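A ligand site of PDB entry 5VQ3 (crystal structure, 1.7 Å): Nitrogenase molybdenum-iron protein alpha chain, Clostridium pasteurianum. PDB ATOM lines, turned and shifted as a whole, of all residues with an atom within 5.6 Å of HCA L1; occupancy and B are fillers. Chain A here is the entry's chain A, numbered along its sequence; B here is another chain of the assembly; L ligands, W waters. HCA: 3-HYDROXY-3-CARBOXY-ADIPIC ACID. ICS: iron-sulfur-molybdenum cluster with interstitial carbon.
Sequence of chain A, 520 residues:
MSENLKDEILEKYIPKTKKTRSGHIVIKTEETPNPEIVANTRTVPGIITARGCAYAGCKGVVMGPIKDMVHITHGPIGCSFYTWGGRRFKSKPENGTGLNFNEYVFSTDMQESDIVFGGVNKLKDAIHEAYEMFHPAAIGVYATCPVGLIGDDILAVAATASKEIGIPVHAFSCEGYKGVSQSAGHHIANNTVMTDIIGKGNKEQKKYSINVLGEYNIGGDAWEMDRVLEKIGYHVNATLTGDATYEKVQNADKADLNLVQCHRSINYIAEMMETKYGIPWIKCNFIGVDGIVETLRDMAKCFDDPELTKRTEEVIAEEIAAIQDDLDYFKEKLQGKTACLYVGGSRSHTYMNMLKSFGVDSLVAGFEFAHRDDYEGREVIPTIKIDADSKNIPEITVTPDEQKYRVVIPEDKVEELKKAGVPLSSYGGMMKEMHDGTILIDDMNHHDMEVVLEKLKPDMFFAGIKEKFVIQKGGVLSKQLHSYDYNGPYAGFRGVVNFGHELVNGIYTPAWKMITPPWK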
ATOM      1  N   GLY A  52     -10.083  31.946  17.845  1.00  0.00           N
ATOM      2  CA  GLY A  52     -11.058  32.872  18.380  1.00  0.00           C
ATOM      3  C   GLY A  52     -10.410  34.207  18.751  1.00  0.00           C
ATOM      4  O   GLY A  52      -9.310  34.533  18.319  1.00  0.00           O
ATOM      5  N   ALA A  56     -13.319  36.016  23.732  1.00  0.00           N
ATOM      6  CA  ALA A  56     -13.546  34.586  24.020  1.00  0.00           C
ATOM      7  C   ALA A  56     -12.589  34.157  25.118  1.00  0.00           C
ATOM      8  O   ALA A  56     -12.980  33.529  26.089  1.00  0.00           O
ATOM      9  CB  ALA A  56     -13.318  33.767  22.792  1.00  0.00           C
ATOM     10  N   GLY A  57     -11.320  34.522  24.961  1.00  0.00           N
ATOM     11  CA  GLY A  57     -10.311  34.157  25.975  1.00  0.00           C
ATOM     12  C   GLY A  57     -10.507  34.706  27.390  1.00  0.00           C
ATOM     13  O   GLY A  57     -10.206  34.051  28.391  1.00  0.00           O
ATOM     14  N   VAL A  61     -13.628  32.082  28.493  1.00  0.00           N
ATOM     15  CA  VAL A  61     -12.722  31.053  28.998  1.00  0.00           C
ATOM     16  C   VAL A  61     -12.352  31.244  30.464  1.00  0.00           C
ATOM     17  O   VAL A  61     -12.712  30.438  31.295  1.00  0.00           O
ATOM     18  CB  VAL A  61     -11.472  30.942  28.121  1.00  0.00           C
ATOM     19  CG1 VAL A  61     -10.445  29.991  28.731  1.00  0.00           C
ATOM     20  CG2 VAL A  61     -11.882  30.498  26.728  1.00  0.00           C
ATOM     21  N   GLY A  86     -21.984  27.016  25.330  1.00  0.00           N
ATOM     22  CA  GLY A  86     -21.209  26.202  24.381  1.00  0.00           C
ATOM     23  C   GLY A  86     -19.944  25.614  24.987  1.00  0.00           C
ATOM     24  O   GLY A  86     -19.532  24.504  24.648  1.00  0.00           O
ATOM     25  N   ARG A  87     -19.358  26.310  25.938  1.00  0.00           N
ATOM     26  CA  ARG A  87     -18.223  25.817  26.701  1.00  0.00           C
ATOM     27  C   ARG A  87     -18.701  25.234  28.038  1.00  0.00           C
ATOM     28  O   ARG A  87     -19.403  25.865  28.830  1.00  0.00           O
ATOM     29  CB  ARG A  87     -17.176  26.926  26.900  1.00  0.00           C
ATOM     30  CG  ARG A  87     -15.941  26.463  27.652  1.00  0.00           C
ATOM     31  CD  ARG A  87     -14.785  27.441  27.434  1.00  0.00           C
ATOM     32  NE  ARG A  87     -13.648  27.130  28.313  1.00  0.00           N
ATOM     33  CZ  ARG A  87     -13.454  27.611  29.549  1.00  0.00           C
ATOM     34  NH1 ARG A  87     -12.334  27.299  30.185  1.00  0.00           N
ATOM     35  NH2 ARG A  87     -14.300  28.437  30.122  1.00  0.00           N
ATOM     36  N   ARG A  88     -18.335  23.987  28.269  1.00  0.00           N
ATOM     37  CA  ARG A  88     -19.059  23.185  29.256  1.00  0.00           C
ATOM     38  C   ARG A  88     -18.474  23.203  30.681  1.00  0.00           C
ATOM     39  O   ARG A  88     -18.329  22.139  31.312  1.00  0.00           O
ATOM     40  CB  ARG A  88     -19.152  21.750  28.731  1.00  0.00           C
ATOM     41  CG  ARG A  88     -19.854  21.652  27.364  1.00  0.00           C
ATOM     42  CD  ARG A  88     -19.985  20.223  26.885  1.00  0.00           C
ATOM     43  NE  ARG A  88     -20.570  19.315  27.853  1.00  0.00           N
ATOM     44  CZ  ARG A  88     -19.922  18.342  28.509  1.00  0.00           C
ATOM     45  NH1 ARG A  88     -20.546  17.613  29.446  1.00  0.00           N
ATOM     46  NH2 ARG A  88     -18.648  18.140  28.297  1.00  0.00           N
ATOM     47  N   GLN A 182      -7.302  33.821  21.338  1.00  0.00           N
ATOM     48  CA  GLN A 182      -7.838  33.775  22.688  1.00  0.00           C
ATOM     49  C   GLN A 182      -6.808  34.084  23.754  1.00  0.00           C
ATOM     50  O   GLN A 182      -7.146  34.552  24.813  1.00  0.00           O
ATOM     51  CB  GLN A 182      -8.387  32.368  22.983  1.00  0.00           C
ATOM     52  CG  GLN A 182      -9.578  31.904  22.145  1.00  0.00           C
ATOM     53  CD  GLN A 182      -9.205  31.142  20.927  1.00  0.00           C
ATOM     54  OE1 GLN A 182      -8.302  31.525  20.165  1.00  0.00           O
ATOM     55  NE2 GLN A 182      -9.910  30.050  20.698  1.00  0.00           N
ATOM     56  N   GLU A 368      -3.984  25.890  18.001  1.00  0.00           N
ATOM     57  CA  GLU A 368      -4.457  27.166  17.483  1.00  0.00           C
ATOM     58  C   GLU A 368      -3.532  28.319  17.888  1.00  0.00           C
ATOM     59  O   GLU A 368      -3.231  29.187  17.061  1.00  0.00           O
ATOM     60  CB  GLU A 368      -5.846  27.498  17.995  1.00  0.00           C
ATOM     61  CG  GLU A 368      -6.938  26.537  17.599  1.00  0.00           C
ATOM     62  CD  GLU A 368      -8.332  26.866  18.200  1.00  0.00           C
ATOM     63  OE1 GLU A 368      -9.226  25.954  18.152  1.00  0.00           O
ATOM     64  OE2 GLU A 368      -8.552  28.017  18.662  1.00  0.00           O
ATOM     65  N   PHE A 369      -3.179  28.410  19.178  1.00  0.00           N
ATOM     66  CA  PHE A 369      -2.656  29.702  19.725  1.00  0.00           C
ATOM     67  C   PHE A 369      -1.598  29.603  20.824  1.00  0.00           C
ATOM     68  O   PHE A 369      -1.300  30.632  21.464  1.00  0.00           O
ATOM     69  CB  PHE A 369      -3.839  30.579  20.220  1.00  0.00           C
ATOM     70  CG  PHE A 369      -4.702  29.915  21.255  1.00  0.00           C
ATOM     71  CD1 PHE A 369      -4.192  29.659  22.530  1.00  0.00           C
ATOM     72  CD2 PHE A 369      -5.948  29.461  20.948  1.00  0.00           C
ATOM     73  CE1 PHE A 369      -4.964  29.001  23.463  1.00  0.00           C
ATOM     74  CE2 PHE A 369      -6.724  28.779  21.875  1.00  0.00           C
ATOM     75  CZ  PHE A 369      -6.224  28.542  23.119  1.00  0.00           C
ATOM     76  N   ALA A 463     -10.164  17.035  17.474  1.00  0.00           N
ATOM     77  CA  ALA A 463     -10.177  18.434  17.199  1.00  0.00           C
ATOM     78  C   ALA A 463     -11.343  19.141  17.940  1.00  0.00           C
ATOM     79  O   ALA A 463     -11.586  18.848  19.098  1.00  0.00           O
ATOM     80  CB  ALA A 463     -10.255  18.661  15.690  1.00  0.00           C
ATOM     81  N   GLY A 464     -12.009  20.064  17.276  1.00  0.00           N
ATOM     82  CA  GLY A 464     -13.129  20.791  17.854  1.00  0.00           C
ATOM     83  C   GLY A 464     -14.332  20.690  16.927  1.00  0.00           C
ATOM     84  O   GLY A 464     -14.361  19.870  16.009  1.00  0.00           O
ATOM     85  N   ILE A 465     -15.358  21.472  17.221  1.00  0.00           N
ATOM     86  CA  ILE A 465     -16.648  21.374  16.568  1.00  0.00           C
ATOM     87  C   ILE A 465     -16.599  21.823  15.074  1.00  0.00           C
ATOM     88  O   ILE A 465     -17.303  21.282  14.258  1.00  0.00           O
ATOM     89  CB  ILE A 465     -17.698  22.189  17.377  1.00  0.00           C
ATOM     90  CG1 ILE A 465     -19.117  21.939  16.872  1.00  0.00           C
ATOM     91  CG2 ILE A 465     -17.388  23.689  17.361  1.00  0.00           C
ATOM     92  CD1 ILE A 465     -19.557  20.515  17.006  1.00  0.00           C
ATOM     93  N   LYS A 466     -15.709  22.752  14.741  1.00  0.00           N
ATOM     94  CA  LYS A 466     -15.646  23.289  13.382  1.00  0.00           C
ATOM     95  C   LYS A 466     -15.022  22.233  12.451  1.00  0.00           C
ATOM     96  O   LYS A 466     -15.372  22.152  11.256  1.00  0.00           O
ATOM     97  CB  LYS A 466     -14.896  24.620  13.332  1.00  0.00           C
ATOM     98  CG  LYS A 466     -15.594  25.737  14.078  1.00  0.00           C
ATOM     99  CD  LYS A 466     -15.011  27.144  13.857  1.00  0.00           C
ATOM    100  CE  LYS A 466     -13.559  27.270  14.223  1.00  0.00           C
ATOM    101  NZ  LYS A 466     -13.170  26.996  15.626  1.00  0.00           N
ATOM    102  N   GLU A 467     -14.126  21.414  13.019  1.00  0.00           N
ATOM    103  CA  GLU A 467     -13.425  20.406  12.225  1.00  0.00           C
ATOM    104  C   GLU A 467     -14.080  19.027  12.286  1.00  0.00           C
ATOM    105  O   GLU A 467     -13.912  18.220  11.374  1.00  0.00           O
ATOM    106  CB  GLU A 467     -12.005  20.258  12.740  1.00  0.00           C
ATOM    107  CG  GLU A 467     -11.185  21.527  12.812  1.00  0.00           C
ATOM    108  CD  GLU A 467     -11.468  22.455  14.015  1.00  0.00           C
ATOM    109  OE1 GLU A 467     -11.998  22.029  15.068  1.00  0.00           O
ATOM    110  OE2 GLU A 467     -11.174  23.671  13.892  1.00  0.00           O
ATOM    111  N   GLN A 480     -14.162  15.189  19.832  1.00  0.00           N
ATOM    112  CA  GLN A 480     -13.864  16.545  20.275  1.00  0.00           C
ATOM    113  C   GLN A 480     -13.042  16.617  21.575  1.00  0.00           C
ATOM    114  O   GLN A 480     -13.443  16.038  22.620  1.00  0.00           O
ATOM    115  CB  GLN A 480     -15.171  17.293  20.490  1.00  0.00           C
ATOM    116  CG  GLN A 480     -15.949  17.549  19.246  1.00  0.00           C
ATOM    117  CD  GLN A 480     -17.218  18.364  19.524  1.00  0.00           C
ATOM    118  OE1 GLN A 480     -17.138  19.563  19.762  1.00  0.00           O
ATOM    119  NE2 GLN A 480     -18.390  17.696  19.521  1.00  0.00           N
ATOM    120  N   HIS A 482     -12.381  19.666  23.031  1.00  0.00           N
ATOM    121  CA  HIS A 482     -12.830  20.783  23.861  1.00  0.00           C
ATOM    122  C   HIS A 482     -14.124  20.405  24.617  1.00  0.00           C
ATOM    123  O   HIS A 482     -14.132  20.398  25.849  1.00  0.00           O
ATOM    124  CB  HIS A 482     -13.125  22.049  23.056  1.00  0.00           C
ATOM    125  CG  HIS A 482     -12.052  22.461  22.101  1.00  0.00           C
ATOM    126  ND1 HIS A 482     -11.384  23.670  22.199  1.00  0.00           N
ATOM    127  CD2 HIS A 482     -11.658  21.921  20.921  1.00  0.00           C
ATOM    128  CE1 HIS A 482     -10.570  23.798  21.171  1.00  0.00           C
ATOM    129  NE2 HIS A 482     -10.718  22.746  20.376  1.00  0.00           N
ATOM    130  N   SER A 483     -15.200  20.135  23.869  1.00  0.00           N
ATOM    131  CA  SER A 483     -16.512  19.851  24.489  1.00  0.00           C
ATOM    132  C   SER A 483     -16.604  18.416  25.017  1.00  0.00           C
ATOM    133  O   SER A 483     -17.571  18.040  25.695  1.00  0.00           O
ATOM    134  CB  SER A 483     -17.585  20.061  23.457  1.00  0.00           C
ATOM    135  OG  SER A 483     -17.546  18.999  22.523  1.00  0.00           O
ATOM    136  N   TYR B  51     -17.296  31.779  15.939  1.00  0.00           N
ATOM    137  CA  TYR B  51     -18.546  31.593  16.629  1.00  0.00           C
ATOM    138  C   TYR B  51     -19.718  31.300  15.652  1.00  0.00           C
ATOM    139  O   TYR B  51     -20.569  30.431  15.917  1.00  0.00           O
ATOM    140  CB  TYR B  51     -18.872  32.811  17.483  1.00  0.00           C
ATOM    141  CG  TYR B  51     -18.200  32.963  18.833  1.00  0.00           C
ATOM    142  CD1 TYR B  51     -17.738  31.893  19.588  1.00  0.00           C
ATOM    143  CD2 TYR B  51     -18.101  34.216  19.392  1.00  0.00           C
ATOM    144  CE1 TYR B  51     -17.235  32.086  20.859  1.00  0.00           C
ATOM    145  CE2 TYR B  51     -17.581  34.406  20.646  1.00  0.00           C
ATOM    146  CZ  TYR B  51     -17.142  33.349  21.386  1.00  0.00           C
ATOM    147  OH  TYR B  51     -16.656  33.568  22.671  1.00  0.00           O
ATOM    148  N   THR B  54     -19.423  27.942  14.192  1.00  0.00           N
ATOM    149  CA  THR B  54     -19.683  26.967  15.245  1.00  0.00           C
ATOM    150  C   THR B  54     -21.177  26.737  15.464  1.00  0.00           C
ATOM    151  O   THR B  54     -21.628  25.577  15.576  1.00  0.00           O
ATOM    152  CB  THR B  54     -18.995  27.384  16.531  1.00  0.00           C
ATOM    153  OG1 THR B  54     -17.582  27.291  16.335  1.00  0.00           O
ATOM    154  CG2 THR B  54     -19.399  26.553  17.730  1.00  0.00           C
ATOM    155  N   ARG B  58     -23.221  23.224  15.159  1.00  0.00           N
ATOM    156  CA  ARG B  58     -23.963  22.692  16.269  1.00  0.00           C
ATOM    157  C   ARG B  58     -25.424  22.401  15.918  1.00  0.00           C
ATOM    158  O   ARG B  58     -26.036  21.470  16.444  1.00  0.00           O
ATOM    159  CB  ARG B  58     -23.853  23.614  17.456  1.00  0.00           C
ATOM    160  CG  ARG B  58     -22.476  23.650  18.115  1.00  0.00           C
ATOM    161  CD  ARG B  58     -22.425  24.712  19.220  1.00  0.00           C
ATOM    162  NE  ARG B  58     -21.181  24.628  19.970  1.00  0.00           N
ATOM    163  CZ  ARG B  58     -20.618  25.611  20.663  1.00  0.00           C
ATOM    164  NH1 ARG B  58     -21.188  26.815  20.715  1.00  0.00           N
ATOM    165  NH2 ARG B  58     -19.439  25.376  21.265  1.00  0.00           N
HETATM  166  C1  HCA L   1     -13.302  29.112  22.470  1.00  0.00           C
HETATM  167  C2  HCA L   1     -14.130  28.059  23.186  1.00  0.00           C
HETATM  168  C3  HCA L   1     -13.804  26.650  22.674  1.00  0.00           C
HETATM  169  C4  HCA L   1     -14.455  26.281  21.334  1.00  0.00           C
HETATM  170  C5  HCA L   1     -14.412  24.754  21.125  1.00  0.00           C
HETATM  171  C6  HCA L   1     -14.523  24.191  19.716  1.00  0.00           C
HETATM  172  C7  HCA L   1     -14.298  25.658  23.714  1.00  0.00           C
HETATM  173  O1  HCA L   1     -13.771  30.283  22.378  1.00  0.00           O
HETATM  174  O2  HCA L   1     -12.225  28.774  21.987  1.00  0.00           O
HETATM  175  O3  HCA L   1     -15.088  23.056  19.577  1.00  0.00           O
HETATM  176  O4  HCA L   1     -14.013  24.812  18.741  1.00  0.00           O
HETATM  177  O5  HCA L   1     -15.516  25.675  24.038  1.00  0.00           O
HETATM  178  O6  HCA L   1     -13.502  24.812  24.218  1.00  0.00           O
HETATM  179  O7  HCA L   1     -12.369  26.510  22.562  1.00  0.00           O
HETATM  180 FE1  ICS L   2      -6.067  26.244  28.424  1.00  0.00          FE
HETATM  181 MO1  ICS L   2     -11.354  25.258  23.956  1.00  0.00          MO
HETATM  182 FE2  ICS L   2      -7.668  27.423  26.633  1.00  0.00          FE
HETATM  183 FE3  ICS L   2      -8.664  25.522  28.229  1.00  0.00          FE
HETATM  184 FE4  ICS L   2      -6.896  24.896  26.313  1.00  0.00          FE
HETATM  185 FE5  ICS L   2      -8.854  24.565  24.657  1.00  0.00          FE
HETATM  186 FE6  ICS L   2      -9.625  27.049  24.993  1.00  0.00          FE
HETATM  187 FE7  ICS L   2     -10.580  25.166  26.516  1.00  0.00          FE
HETATM  188  CX  ICS L   2      -8.670  25.723  26.216  1.00  0.00           C
HETATM  189  S1A ICS L   2      -5.537  26.735  26.275  1.00  0.00           S
HETATM  190  S1B ICS L   2      -9.336  26.065  23.036  1.00  0.00           S
HETATM  191  S2A ICS L   2      -7.848  27.585  28.845  1.00  0.00           S
HETATM  192  S2B ICS L   2      -8.647  28.967  25.347  1.00  0.00           S
HETATM  193  S3A ICS L   2      -6.909  23.496  24.632  1.00  0.00           S
HETATM  194  S3B ICS L   2     -11.715  26.876  25.650  1.00  0.00           S
HETATM  195  S4A ICS L   2      -6.919  24.099  28.452  1.00  0.00           S
HETATM  196  S4B ICS L   2     -10.691  23.375  25.199  1.00  0.00           S
HETATM  197  S5A ICS L   2     -10.743  24.840  28.690  1.00  0.00           S
HETATM  198  O   HOH W   1     -17.548  23.041  21.077  1.00  0.00           O
HETATM  199  O   HOH W   2     -11.729  26.595  18.807  1.00  0.00           O
HETATM  200  O   HOH W   3     -15.904  31.353  23.967  1.00  0.00           O
HETATM  201  O   HOH W   4     -13.567  24.168  16.326  1.00  0.00           O
HETATM  202  O   HOH W   5     -14.059  23.667  26.727  1.00  0.00           O
HETATM  203  O   HOH W   6     -13.518  31.327  19.960  1.00  0.00           O
HETATM  204  O   HOH W   7     -15.218  27.142  17.709  1.00  0.00           O
HETATM  205  O   HOH W   8     -14.944  20.601  20.867  1.00  0.00           O
HETATM  206  O   HOH W   9     -17.085  23.565  23.785  1.00  0.00           O
HETATM  207  O   HOH W  10     -17.797  27.173  22.965  1.00  0.00           O
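O7 of HCA L1 is bound to MO1 of ICS L2 (2.1 Å).
The guanidinium group of Arg 87 lies close to a sulfur (S5A) of ICS L2, at 3.3 Å. The side-chain amino group (NZ) of Lys 466 lies within salt-bridge range of an oxygen (O4) of HCA L1 (3.9 Å). ND1 of His 482 is bound to MO1 of ICS L2 (2.4 Å). N of Ile 465 sits at hydrogen-bond distance from O3 of HCA L1 (2.9 Å). The side-chain amide nitrogen (NE2) of Gln 182 sits at hydrogen-bond distance from an oxygen (O2) of HCA L1.
OE1 of Gln 182 lies within hydrogen-bond range of N of Gly 52. The backbone NH (N) of Gly 464 sits at hydrogen-bond distance from the side-chain carboxylate (OE1) of Glu 467 (3.0 Å). NH2 of Arg 87 sits at hydrogen-bond distance from O of Val 61 (2.8 Å). The side-chain amide nitrogen (NE2) of Gln 182 sits at hydrogen-bond distance from the side-chain carboxylate (OE2) of Glu 368. The backbone carbonyl oxygen (O) of Ala 56 is in hydrogen-bond range of the backbone NH (N) of Val 61 (2.9 Å).
A ring nitrogen (ND1) of His 482 lies close to an oxygen (O7) of HCA L1, at 3.0 Å. Merely in contact with HCA L1: Gly 464, Arg 87 and Ala 56. Hydrophobic or aromatic side chains that line HCA L1: Ala 56, Ile 465 and His 482. The nearest printed residue that does not touch HCA L1 is Gln 480 (4.1 Å).
Water W4 lies within hydrogen-bond range of an oxygen (O4) of HCA L1 (2.5 Å), the side-chain carboxylate (OE1) of Glu 467 (2.9 Å), the side-chain amino group (NZ) of Lys 466 (2.9 Å) and the backbone NH (N) of Ile 465 (3.4 Å). Water W9 bridges an oxygen (O5) of HCA L1 (2.6 Å) and the backbone carbonyl oxygen (O) of Gly 86 (2.8 Å). Water W7 lies within hydrogen-bond range of OG1 of Thr 54 of chain B (2.7 Å), O4 of HCA L1 (2.8 Å) and NZ of Lys 466 (2.9 Å). Water W3 bridges OH of Tyr 51 of chain B (2.7 Å) and O1 of HCA L1 (2.9 Å). Water W2 bridges the side-chain carboxylate (OE1) of Glu 368 (2.7 Å) and an oxygen (O4) of HCA L1 (2.9 Å). Water W10 lies within hydrogen-bond range of O5 of HCA L1 (2.9 Å), NH2 of Arg 58 of chain B (3.0 Å) and N of Arg 87 (3.5 Å).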
